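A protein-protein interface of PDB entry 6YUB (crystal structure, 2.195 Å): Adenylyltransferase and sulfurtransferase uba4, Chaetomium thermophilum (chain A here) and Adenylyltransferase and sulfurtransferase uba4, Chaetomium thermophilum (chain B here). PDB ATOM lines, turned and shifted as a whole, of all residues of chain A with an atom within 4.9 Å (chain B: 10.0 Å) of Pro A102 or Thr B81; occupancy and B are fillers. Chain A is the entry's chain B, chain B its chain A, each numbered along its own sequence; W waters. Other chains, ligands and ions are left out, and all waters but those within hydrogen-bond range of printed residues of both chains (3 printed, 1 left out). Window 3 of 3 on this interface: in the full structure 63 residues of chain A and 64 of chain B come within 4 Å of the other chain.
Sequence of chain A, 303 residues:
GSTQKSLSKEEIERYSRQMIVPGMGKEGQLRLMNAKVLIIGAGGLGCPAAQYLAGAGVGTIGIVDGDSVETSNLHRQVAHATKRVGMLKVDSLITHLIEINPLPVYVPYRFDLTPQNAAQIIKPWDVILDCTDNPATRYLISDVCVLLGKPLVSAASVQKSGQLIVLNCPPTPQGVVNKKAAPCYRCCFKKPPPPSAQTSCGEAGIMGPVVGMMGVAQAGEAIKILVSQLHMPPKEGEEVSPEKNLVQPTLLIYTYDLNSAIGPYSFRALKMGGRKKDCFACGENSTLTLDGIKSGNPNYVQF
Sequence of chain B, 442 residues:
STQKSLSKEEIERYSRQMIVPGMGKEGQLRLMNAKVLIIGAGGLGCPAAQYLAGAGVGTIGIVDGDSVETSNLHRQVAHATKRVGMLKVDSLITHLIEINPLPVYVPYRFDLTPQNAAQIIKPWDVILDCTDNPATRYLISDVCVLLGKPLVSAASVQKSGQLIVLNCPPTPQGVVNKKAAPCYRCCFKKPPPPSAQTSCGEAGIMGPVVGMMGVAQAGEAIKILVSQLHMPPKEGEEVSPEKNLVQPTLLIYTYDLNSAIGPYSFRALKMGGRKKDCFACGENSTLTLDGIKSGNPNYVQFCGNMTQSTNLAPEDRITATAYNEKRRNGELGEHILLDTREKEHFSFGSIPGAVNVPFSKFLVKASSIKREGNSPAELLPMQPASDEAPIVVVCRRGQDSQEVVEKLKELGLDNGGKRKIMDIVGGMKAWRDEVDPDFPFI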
ATOM      1  N   ARG A  14      22.899 -26.236  27.615  1.00  0.00           N
ATOM      2  CA  ARG A  14      24.221 -26.257  27.001  1.00  0.00           C
ATOM      3  C   ARG A  14      24.906 -27.610  27.161  1.00  0.00           C
ATOM      4  O   ARG A  14      25.622 -28.044  26.250  1.00  0.00           O
ATOM      5  CB  ARG A  14      25.083 -25.134  27.600  1.00  0.00           C
ATOM      6  CG  ARG A  14      26.464 -24.993  26.993  1.00  0.00           C
ATOM      7  CD  ARG A  14      27.200 -23.768  27.547  1.00  0.00           C
ATOM      8  NE  ARG A  14      26.907 -22.555  26.793  1.00  0.00           N
ATOM      9  CZ  ARG A  14      27.585 -22.160  25.717  1.00  0.00           C
ATOM     10  NH1 ARG A  14      28.607 -22.878  25.262  1.00  0.00           N
ATOM     11  NH2 ARG A  14      27.244 -21.044  25.096  1.00  0.00           N
ATOM     12  N   LEU A  97      37.992 -19.266  23.184  1.00  0.00           N
ATOM     13  CA  LEU A  97      37.297 -20.029  24.216  1.00  0.00           C
ATOM     14  C   LEU A  97      36.013 -19.326  24.635  1.00  0.00           C
ATOM     15  O   LEU A  97      34.969 -19.965  24.791  1.00  0.00           O
ATOM     16  CB  LEU A  97      38.212 -20.241  25.423  1.00  0.00           C
ATOM     17  CG  LEU A  97      39.523 -20.981  25.161  1.00  0.00           C
ATOM     18  CD1 LEU A  97      40.329 -21.108  26.452  1.00  0.00           C
ATOM     19  CD2 LEU A  97      39.286 -22.350  24.548  1.00  0.00           C
ATOM     20  N   ILE A  98      36.072 -18.006  24.826  1.00  0.00           N
ATOM     21  CA  ILE A  98      34.875 -17.248  25.174  1.00  0.00           C
ATOM     22  C   ILE A  98      33.815 -17.399  24.089  1.00  0.00           C
ATOM     23  O   ILE A  98      32.616 -17.458  24.381  1.00  0.00           O
ATOM     24  CB  ILE A  98      35.237 -15.773  25.423  1.00  0.00           C
ATOM     25  CG1 ILE A  98      35.992 -15.648  26.754  1.00  0.00           C
ATOM     26  CG2 ILE A  98      33.987 -14.899  25.417  1.00  0.00           C
ATOM     27  CD1 ILE A  98      36.661 -14.312  26.958  1.00  0.00           C
ATOM     28  N   GLU A  99      34.238 -17.478  22.825  1.00  0.00           N
ATOM     29  CA  GLU A  99      33.293 -17.750  21.750  1.00  0.00           C
ATOM     30  C   GLU A  99      32.628 -19.105  21.935  1.00  0.00           C
ATOM     31  O   GLU A  99      31.406 -19.234  21.777  1.00  0.00           O
ATOM     32  CB  GLU A  99      33.999 -17.688  20.396  1.00  0.00           C
ATOM     33  CG  GLU A  99      34.404 -16.288  19.959  1.00  0.00           C
ATOM     34  CD  GLU A  99      35.019 -16.273  18.570  1.00  0.00           C
ATOM     35  OE1 GLU A  99      35.722 -17.240  18.220  1.00  0.00           O
ATOM     36  OE2 GLU A  99      34.787 -15.298  17.823  1.00  0.00           O
ATOM     37  N   ILE A 100      33.420 -20.133  22.271  1.00  0.00           N
ATOM     38  CA  ILE A 100      32.882 -21.478  22.426  1.00  0.00           C
ATOM     39  C   ILE A 100      31.910 -21.529  23.598  1.00  0.00           C
ATOM     40  O   ILE A 100      30.824 -22.120  23.508  1.00  0.00           O
ATOM     41  CB  ILE A 100      34.027 -22.491  22.612  1.00  0.00           C
ATOM     42  CG1 ILE A 100      34.877 -22.574  21.344  1.00  0.00           C
ATOM     43  CG2 ILE A 100      33.471 -23.864  23.000  1.00  0.00           C
ATOM     44  CD1 ILE A 100      36.132 -23.407  21.515  1.00  0.00           C
ATOM     45  N   ASN A 101      32.295 -20.927  24.719  1.00  0.00           N
ATOM     46  CA  ASN A 101      31.535 -21.025  25.956  1.00  0.00           C
ATOM     47  C   ASN A 101      31.927 -19.881  26.883  1.00  0.00           C
ATOM     48  O   ASN A 101      33.039 -19.880  27.431  1.00  0.00           O
ATOM     49  CB  ASN A 101      31.794 -22.373  26.630  1.00  0.00           C
ATOM     50  CG  ASN A 101      30.836 -22.650  27.763  1.00  0.00           C
ATOM     51  OD1 ASN A 101      30.056 -21.779  28.163  1.00  0.00           O
ATOM     52  ND2 ASN A 101      30.888 -23.867  28.295  1.00  0.00           N
ATOM     53  N   PRO A 102      31.061 -18.883  27.072  1.00  0.00           N
ATOM     54  CA  PRO A 102      31.396 -17.757  27.956  1.00  0.00           C
ATOM     55  C   PRO A 102      31.092 -17.980  29.430  1.00  0.00           C
ATOM     56  O   PRO A 102      31.293 -17.056  30.223  1.00  0.00           O
ATOM     57  CB  PRO A 102      30.516 -16.624  27.394  1.00  0.00           C
ATOM     58  CG  PRO A 102      29.287 -17.337  26.900  1.00  0.00           C
ATOM     59  CD  PRO A 102      29.769 -18.681  26.378  1.00  0.00           C
ATOM     60  N   LEU A 103      30.622 -19.158  29.820  1.00  0.00           N
ATOM     61  CA  LEU A 103      30.242 -19.388  31.208  1.00  0.00           C
ATOM     62  C   LEU A 103      31.445 -19.668  32.108  1.00  0.00           C
ATOM     63  O   LEU A 103      31.441 -19.255  33.276  1.00  0.00           O
ATOM     64  CB  LEU A 103      29.238 -20.544  31.294  1.00  0.00           C
ATOM     65  CG  LEU A 103      27.946 -20.352  30.505  1.00  0.00           C
ATOM     66  CD1 LEU A 103      26.943 -21.445  30.828  1.00  0.00           C
ATOM     67  CD2 LEU A 103      27.333 -18.981  30.771  1.00  0.00           C
ATOM     68  N   PRO A 104      32.484 -20.352  31.632  1.00  0.00           N
ATOM     69  CA  PRO A 104      33.645 -20.600  32.497  1.00  0.00           C
ATOM     70  C   PRO A 104      34.445 -19.330  32.748  1.00  0.00           C
ATOM     71  O   PRO A 104      34.396 -18.365  31.985  1.00  0.00           O
ATOM     72  CB  PRO A 104      34.478 -21.625  31.711  1.00  0.00           C
ATOM     73  CG  PRO A 104      33.573 -22.158  30.655  1.00  0.00           C
ATOM     74  CD  PRO A 104      32.611 -21.050  30.339  1.00  0.00           C
ATOM     75  N   VAL B  68      23.647 -23.731  13.730  1.00  0.00           N
ATOM     76  CA  VAL B  68      24.392 -23.782  14.981  1.00  0.00           C
ATOM     77  C   VAL B  68      23.425 -23.688  16.152  1.00  0.00           C
ATOM     78  O   VAL B  68      22.569 -22.795  16.199  1.00  0.00           O
ATOM     79  CB  VAL B  68      25.437 -22.652  15.035  1.00  0.00           C
ATOM     80  CG1 VAL B  68      26.135 -22.625  16.397  1.00  0.00           C
ATOM     81  CG2 VAL B  68      26.463 -22.807  13.915  1.00  0.00           C
ATOM     82  N   GLU B  69      23.569 -24.600  17.111  1.00  0.00           N
ATOM     83  CA  GLU B  69      22.726 -24.636  18.297  1.00  0.00           C
ATOM     84  C   GLU B  69      23.597 -24.621  19.546  1.00  0.00           C
ATOM     85  O   GLU B  69      24.696 -25.178  19.562  1.00  0.00           O
ATOM     86  CB  GLU B  69      21.819 -25.878  18.302  1.00  0.00           C
ATOM     87  CG  GLU B  69      20.977 -26.033  17.046  1.00  0.00           C
ATOM     88  CD  GLU B  69      20.160 -27.314  17.041  1.00  0.00           C
ATOM     89  OE1 GLU B  69      19.593 -27.664  18.096  1.00  0.00           O
ATOM     90  OE2 GLU B  69      20.093 -27.975  15.984  1.00  0.00           O
ATOM     91  N   THR B  70      23.085 -23.977  20.597  1.00  0.00           N
ATOM     92  CA  THR B  70      23.834 -23.859  21.841  1.00  0.00           C
ATOM     93  C   THR B  70      24.170 -25.229  22.421  1.00  0.00           C
ATOM     94  O   THR B  70      25.250 -25.424  22.988  1.00  0.00           O
ATOM     95  CB  THR B  70      23.034 -23.040  22.855  1.00  0.00           C
ATOM     96  OG1 THR B  70      22.622 -21.802  22.261  1.00  0.00           O
ATOM     97  CG2 THR B  70      23.873 -22.756  24.107  1.00  0.00           C
ATOM     98  N   SER B  71      23.257 -26.193  22.280  1.00  0.00           N
ATOM     99  CA  SER B  71      23.436 -27.489  22.918  1.00  0.00           C
ATOM    100  C   SER B  71      24.524 -28.332  22.271  1.00  0.00           C
ATOM    101  O   SER B  71      24.892 -29.365  22.835  1.00  0.00           O
ATOM    102  CB  SER B  71      22.107 -28.251  22.905  1.00  0.00           C
ATOM    103  OG  SER B  71      21.648 -28.444  21.583  1.00  0.00           O
ATOM    104  N   ASN B  72      25.047 -27.926  21.119  1.00  0.00           N
ATOM    105  CA  ASN B  72      26.083 -28.681  20.427  1.00  0.00           C
ATOM    106  C   ASN B  72      27.451 -28.007  20.476  1.00  0.00           C
ATOM    107  O   ASN B  72      28.422 -28.572  19.960  1.00  0.00           O
ATOM    108  CB  ASN B  72      25.674 -28.906  18.965  1.00  0.00           C
ATOM    109  CG  ASN B  72      24.326 -29.607  18.837  1.00  0.00           C
ATOM    110  OD1 ASN B  72      23.950 -30.404  19.692  1.00  0.00           O
ATOM    111  ND2 ASN B  72      23.595 -29.305  17.766  1.00  0.00           N
ATOM    112  N   LEU B  73      27.556 -26.816  21.075  1.00  0.00           N
ATOM    113  CA  LEU B  73      28.833 -26.107  21.099  1.00  0.00           C
ATOM    114  C   LEU B  73      29.884 -26.853  21.907  1.00  0.00           C
ATOM    115  O   LEU B  73      31.083 -26.683  21.663  1.00  0.00           O
ATOM    116  CB  LEU B  73      28.647 -24.696  21.665  1.00  0.00           C
ATOM    117  CG  LEU B  73      27.785 -23.747  20.832  1.00  0.00           C
ATOM    118  CD1 LEU B  73      27.472 -22.481  21.620  1.00  0.00           C
ATOM    119  CD2 LEU B  73      28.475 -23.401  19.515  1.00  0.00           C
ATOM    120  N   HIS B  74      29.464 -27.677  22.871  1.00  0.00           N
ATOM    121  CA  HIS B  74      30.424 -28.410  23.689  1.00  0.00           C
ATOM    122  C   HIS B  74      31.310 -29.328  22.860  1.00  0.00           C
ATOM    123  O   HIS B  74      32.419 -29.665  23.297  1.00  0.00           O
ATOM    124  CB  HIS B  74      29.692 -29.225  24.754  1.00  0.00           C
ATOM    125  CG  HIS B  74      29.056 -30.478  24.230  1.00  0.00           C
ATOM    126  ND1 HIS B  74      29.544 -31.735  24.519  1.00  0.00           N
ATOM    127  CD2 HIS B  74      27.976 -30.665  23.433  1.00  0.00           C
ATOM    128  CE1 HIS B  74      28.788 -32.642  23.925  1.00  0.00           C
ATOM    129  NE2 HIS B  74      27.833 -32.020  23.257  1.00  0.00           N
ATOM    130  N   GLN B  76      31.278 -28.915  19.077  1.00  0.00           N
ATOM    131  CA  GLN B  76      31.466 -28.266  17.780  1.00  0.00           C
ATOM    132  C   GLN B  76      32.237 -26.973  18.040  1.00  0.00           C
ATOM    133  O   GLN B  76      31.684 -25.868  17.997  1.00  0.00           O
ATOM    134  CB  GLN B  76      30.114 -28.010  17.089  1.00  0.00           C
ATOM    135  CG  GLN B  76      29.281 -29.262  16.913  1.00  0.00           C
ATOM    136  CD  GLN B  76      27.968 -29.016  16.188  1.00  0.00           C
ATOM    137  OE1 GLN B  76      27.606 -27.874  15.888  1.00  0.00           O
ATOM    138  NE2 GLN B  76      27.248 -30.094  15.895  1.00  0.00           N
ATOM    139  N   VAL B  77      33.540 -27.123  18.299  1.00  0.00           N
ATOM    140  CA  VAL B  77      34.348 -26.037  18.851  1.00  0.00           C
ATOM    141  C   VAL B  77      34.798 -25.025  17.816  1.00  0.00           C
ATOM    142  O   VAL B  77      35.483 -24.060  18.174  1.00  0.00           O
ATOM    143  CB  VAL B  77      35.588 -26.616  19.571  1.00  0.00           C
ATOM    144  CG1 VAL B  77      35.163 -27.587  20.660  1.00  0.00           C
ATOM    145  CG2 VAL B  77      36.525 -27.296  18.577  1.00  0.00           C
ATOM    146  N   ALA B  78      34.451 -25.213  16.547  1.00  0.00           N
ATOM    147  CA  ALA B  78      34.711 -24.201  15.534  1.00  0.00           C
ATOM    148  C   ALA B  78      33.605 -23.155  15.454  1.00  0.00           C
ATOM    149  O   ALA B  78      33.791 -22.124  14.801  1.00  0.00           O
ATOM    150  CB  ALA B  78      34.889 -24.851  14.158  1.00  0.00           C
ATOM    151  N   HIS B  79      32.466 -23.401  16.091  1.00  0.00           N
ATOM    152  CA  HIS B  79      31.360 -22.462  16.101  1.00  0.00           C
ATOM    153  C   HIS B  79      31.477 -21.526  17.300  1.00  0.00           C
ATOM    154  O   HIS B  79      32.258 -21.754  18.230  1.00  0.00           O
ATOM    155  CB  HIS B  79      30.028 -23.212  16.124  1.00  0.00           C
ATOM    156  CG  HIS B  79      29.815 -24.091  14.932  1.00  0.00           C
ATOM    157  ND1 HIS B  79      30.127 -23.696  13.648  1.00  0.00           N
ATOM    158  CD2 HIS B  79      29.339 -25.354  14.828  1.00  0.00           C
ATOM    159  CE1 HIS B  79      29.845 -24.673  12.806  1.00  0.00           C
ATOM    160  NE2 HIS B  79      29.364 -25.691  13.497  1.00  0.00           N
ATOM    161  N   ALA B  80      30.698 -20.452  17.262  1.00  0.00           N
ATOM    162  CA  ALA B  80      30.710 -19.436  18.302  1.00  0.00           C
ATOM    163  C   ALA B  80      29.311 -19.266  18.875  1.00  0.00           C
ATOM    164  O   ALA B  80      28.312 -19.455  18.178  1.00  0.00           O
ATOM    165  CB  ALA B  80      31.218 -18.091  17.762  1.00  0.00           C
ATOM    166  N   THR B  81      29.250 -18.918  20.162  1.00  0.00           N
ATOM    167  CA  THR B  81      27.967 -18.622  20.786  1.00  0.00           C
ATOM    168  C   THR B  81      27.262 -17.480  20.061  1.00  0.00           C
ATOM    169  O   THR B  81      26.038 -17.500  19.900  1.00  0.00           O
ATOM    170  CB  THR B  81      28.169 -18.281  22.265  1.00  0.00           C
ATOM    171  OG1 THR B  81      28.680 -19.426  22.958  1.00  0.00           O
ATOM    172  CG2 THR B  81      26.861 -17.846  22.908  1.00  0.00           C
ATOM    173  N   LYS B  82      28.025 -16.480  19.607  1.00  0.00           N
ATOM    174  CA  LYS B  82      27.450 -15.371  18.861  1.00  0.00           C
ATOM    175  C   LYS B  82      26.852 -15.817  17.531  1.00  0.00           C
ATOM    176  O   LYS B  82      26.018 -15.101  16.966  1.00  0.00           O
ATOM    177  CB  LYS B  82      28.504 -14.293  18.595  1.00  0.00           C
ATOM    178  CG  LYS B  82      29.019 -13.587  19.832  1.00  0.00           C
ATOM    179  CD  LYS B  82      29.990 -12.436  19.494  1.00  0.00           C
ATOM    180  CE  LYS B  82      30.889 -12.740  18.286  1.00  0.00           C
ATOM    181  NZ  LYS B  82      31.725 -13.973  18.441  1.00  0.00           N
ATOM    182  N   ARG B  83      27.263 -16.982  17.018  1.00  0.00           N
ATOM    183  CA  ARG B  83      26.808 -17.466  15.724  1.00  0.00           C
ATOM    184  C   ARG B  83      25.757 -18.565  15.846  1.00  0.00           C
ATOM    185  O   ARG B  83      25.497 -19.274  14.866  1.00  0.00           O
ATOM    186  CB  ARG B  83      27.992 -17.961  14.894  1.00  0.00           C
ATOM    187  CG  ARG B  83      29.009 -16.867  14.566  1.00  0.00           C
ATOM    188  CD  ARG B  83      29.920 -17.249  13.400  1.00  0.00           C
ATOM    189  NE  ARG B  83      30.820 -18.356  13.712  1.00  0.00           N
ATOM    190  CZ  ARG B  83      32.034 -18.218  14.250  1.00  0.00           C
ATOM    191  NH1 ARG B  83      32.498 -17.019  14.562  1.00  0.00           N
ATOM    192  NH2 ARG B  83      32.786 -19.288  14.483  1.00  0.00           N
ATOM    193  N   VAL B  84      25.149 -18.723  17.026  1.00  0.00           N
ATOM    194  CA  VAL B  84      23.988 -19.597  17.150  1.00  0.00           C
ATOM    195  C   VAL B  84      22.867 -19.072  16.263  1.00  0.00           C
ATOM    196  O   VAL B  84      22.577 -17.869  16.244  1.00  0.00           O
ATOM    197  CB  VAL B  84      23.547 -19.686  18.618  1.00  0.00           C
ATOM    198  CG1 VAL B  84      22.183 -20.348  18.728  1.00  0.00           C
ATOM    199  CG2 VAL B  84      24.580 -20.462  19.432  1.00  0.00           C
ATOM    200  N   GLY B  85      22.222 -19.978  15.530  1.00  0.00           N
ATOM    201  CA  GLY B  85      21.202 -19.628  14.570  1.00  0.00           C
ATOM    202  C   GLY B  85      21.696 -19.539  13.142  1.00  0.00           C
ATOM    203  O   GLY B  85      20.891 -19.645  12.212  1.00  0.00           O
ATOM    204  N   MET B  86      22.998 -19.349  12.949  1.00  0.00           N
ATOM    205  CA  MET B  86      23.595 -19.325  11.624  1.00  0.00           C
ATOM    206  C   MET B  86      23.752 -20.744  11.097  1.00  0.00           C
ATOM    207  O   MET B  86      23.869 -21.705  11.862  1.00  0.00           O
ATOM    208  CB  MET B  86      24.956 -18.626  11.680  1.00  0.00           C
ATOM    209  CG  MET B  86      25.664 -18.468  10.346  1.00  0.00           C
ATOM    210  SD  MET B  86      27.242 -17.569  10.502  1.00  0.00           S
ATOM    211  CE  MET B  86      26.705 -16.043  11.253  1.00  0.00           C
ATOM    212  N   SER B  91      28.950 -20.650   9.617  1.00  0.00           N
ATOM    213  CA  SER B  91      29.677 -20.457  10.866  1.00  0.00           C
ATOM    214  C   SER B  91      31.086 -21.032  10.781  1.00  0.00           C
ATOM    215  O   SER B  91      32.049 -20.402  11.237  1.00  0.00           O
ATOM    216  CB  SER B  91      28.910 -21.107  12.020  1.00  0.00           C
ATOM    217  OG  SER B  91      29.577 -20.910  13.252  1.00  0.00           O
HETATM  218  O   HOH W   1      29.163 -25.858  25.823  1.00  0.00           O
HETATM  219  O   HOH W   2      34.689 -15.129  15.252  1.00  0.00           O
HETATM  220  O   HOH W   3      35.589 -18.293  15.647  1.00  0.00           O
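The backbone NH (N) of Thr B81 sits at hydrogen-bond distance from the backbone carbonyl oxygen (O) of Glu A99 (2.7 Å). OG1 of Thr B81 lies within hydrogen-bond range of NH2 of Arg A14 (3.0 Å). The side-chain amino group (NZ) of Lys B82 is in salt-bridge range of the side-chain carboxylate (OE2) of Glu A99 (3.4 Å). The side-chain hydroxyl (OG1) of Thr B81 sits at hydrogen-bond distance from the backbone carbonyl oxygen (O) of Ile A100.
The side-chain amide oxygen (OD1) of Asn A101 lies close to the guanidinium group (NH1) of Arg A14 (3.4 Å). NH1 of Arg A14 is in hydrogen-bond range of O of Ile A100 (2.9 Å).
Among the printed residues, merely in contact across the chains: Ile A100 with Val B77, Glu A99 with Ala B80, Pro A102 with Thr B81, Arg A14 with Ser B71, Arg A14 with Leu B73, Ile A100 with Leu B73 and Arg A14 with Thr B70.
Pro A102 touches just one residue of chain B: Thr B81. Thr B81 touches just these residues of chain A: Arg A14, Glu A99, Ile A100 and Pro A102. No residue of chain B comes within 4 Å of Leu A103. No residue of chain B comes within 4 Å of Pro A104. Of the printed residues of chain A, Ser B71 touches Arg A14 (3.7 Å). Of the printed residues of chain B, Ile A100 touches Leu B73 (3.8 Å), Val B77 (3.5 Å) and Thr B81 (3.5 Å). Printed residues of chain A within 4 Å of Ala B80: Glu A99. Printed residues of chain A within 4 Å of Thr B70: Arg A14 (3.9 Å). The nearest residue of chain A that does not touch Thr B81 is Asn A101 (4.3 Å). The nearest printed residue of chain A that does not touch Thr B70 is Ile A100 (6.5 Å).
Among the printed residues, Asp or Glu carboxylates within 4 Å of a Lys or Arg side-chain nitrogen of the other chain: Glu A99 with Lys B82 (3.4 Å).
Water W2 bridges the side-chain carboxylate (OE2) of Glu A99 (2.6 Å) and the guanidinium group (NH1) of Arg B83 (3.0 Å). Water W3 lies within hydrogen-bond range of the side-chain carboxylate of Glu A99 and the guanidinium group of Arg B83. Water W1 lies within hydrogen-bond range of the guanidinium group (NH1) of Arg A14 and the backbone NH (N) of His B74.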
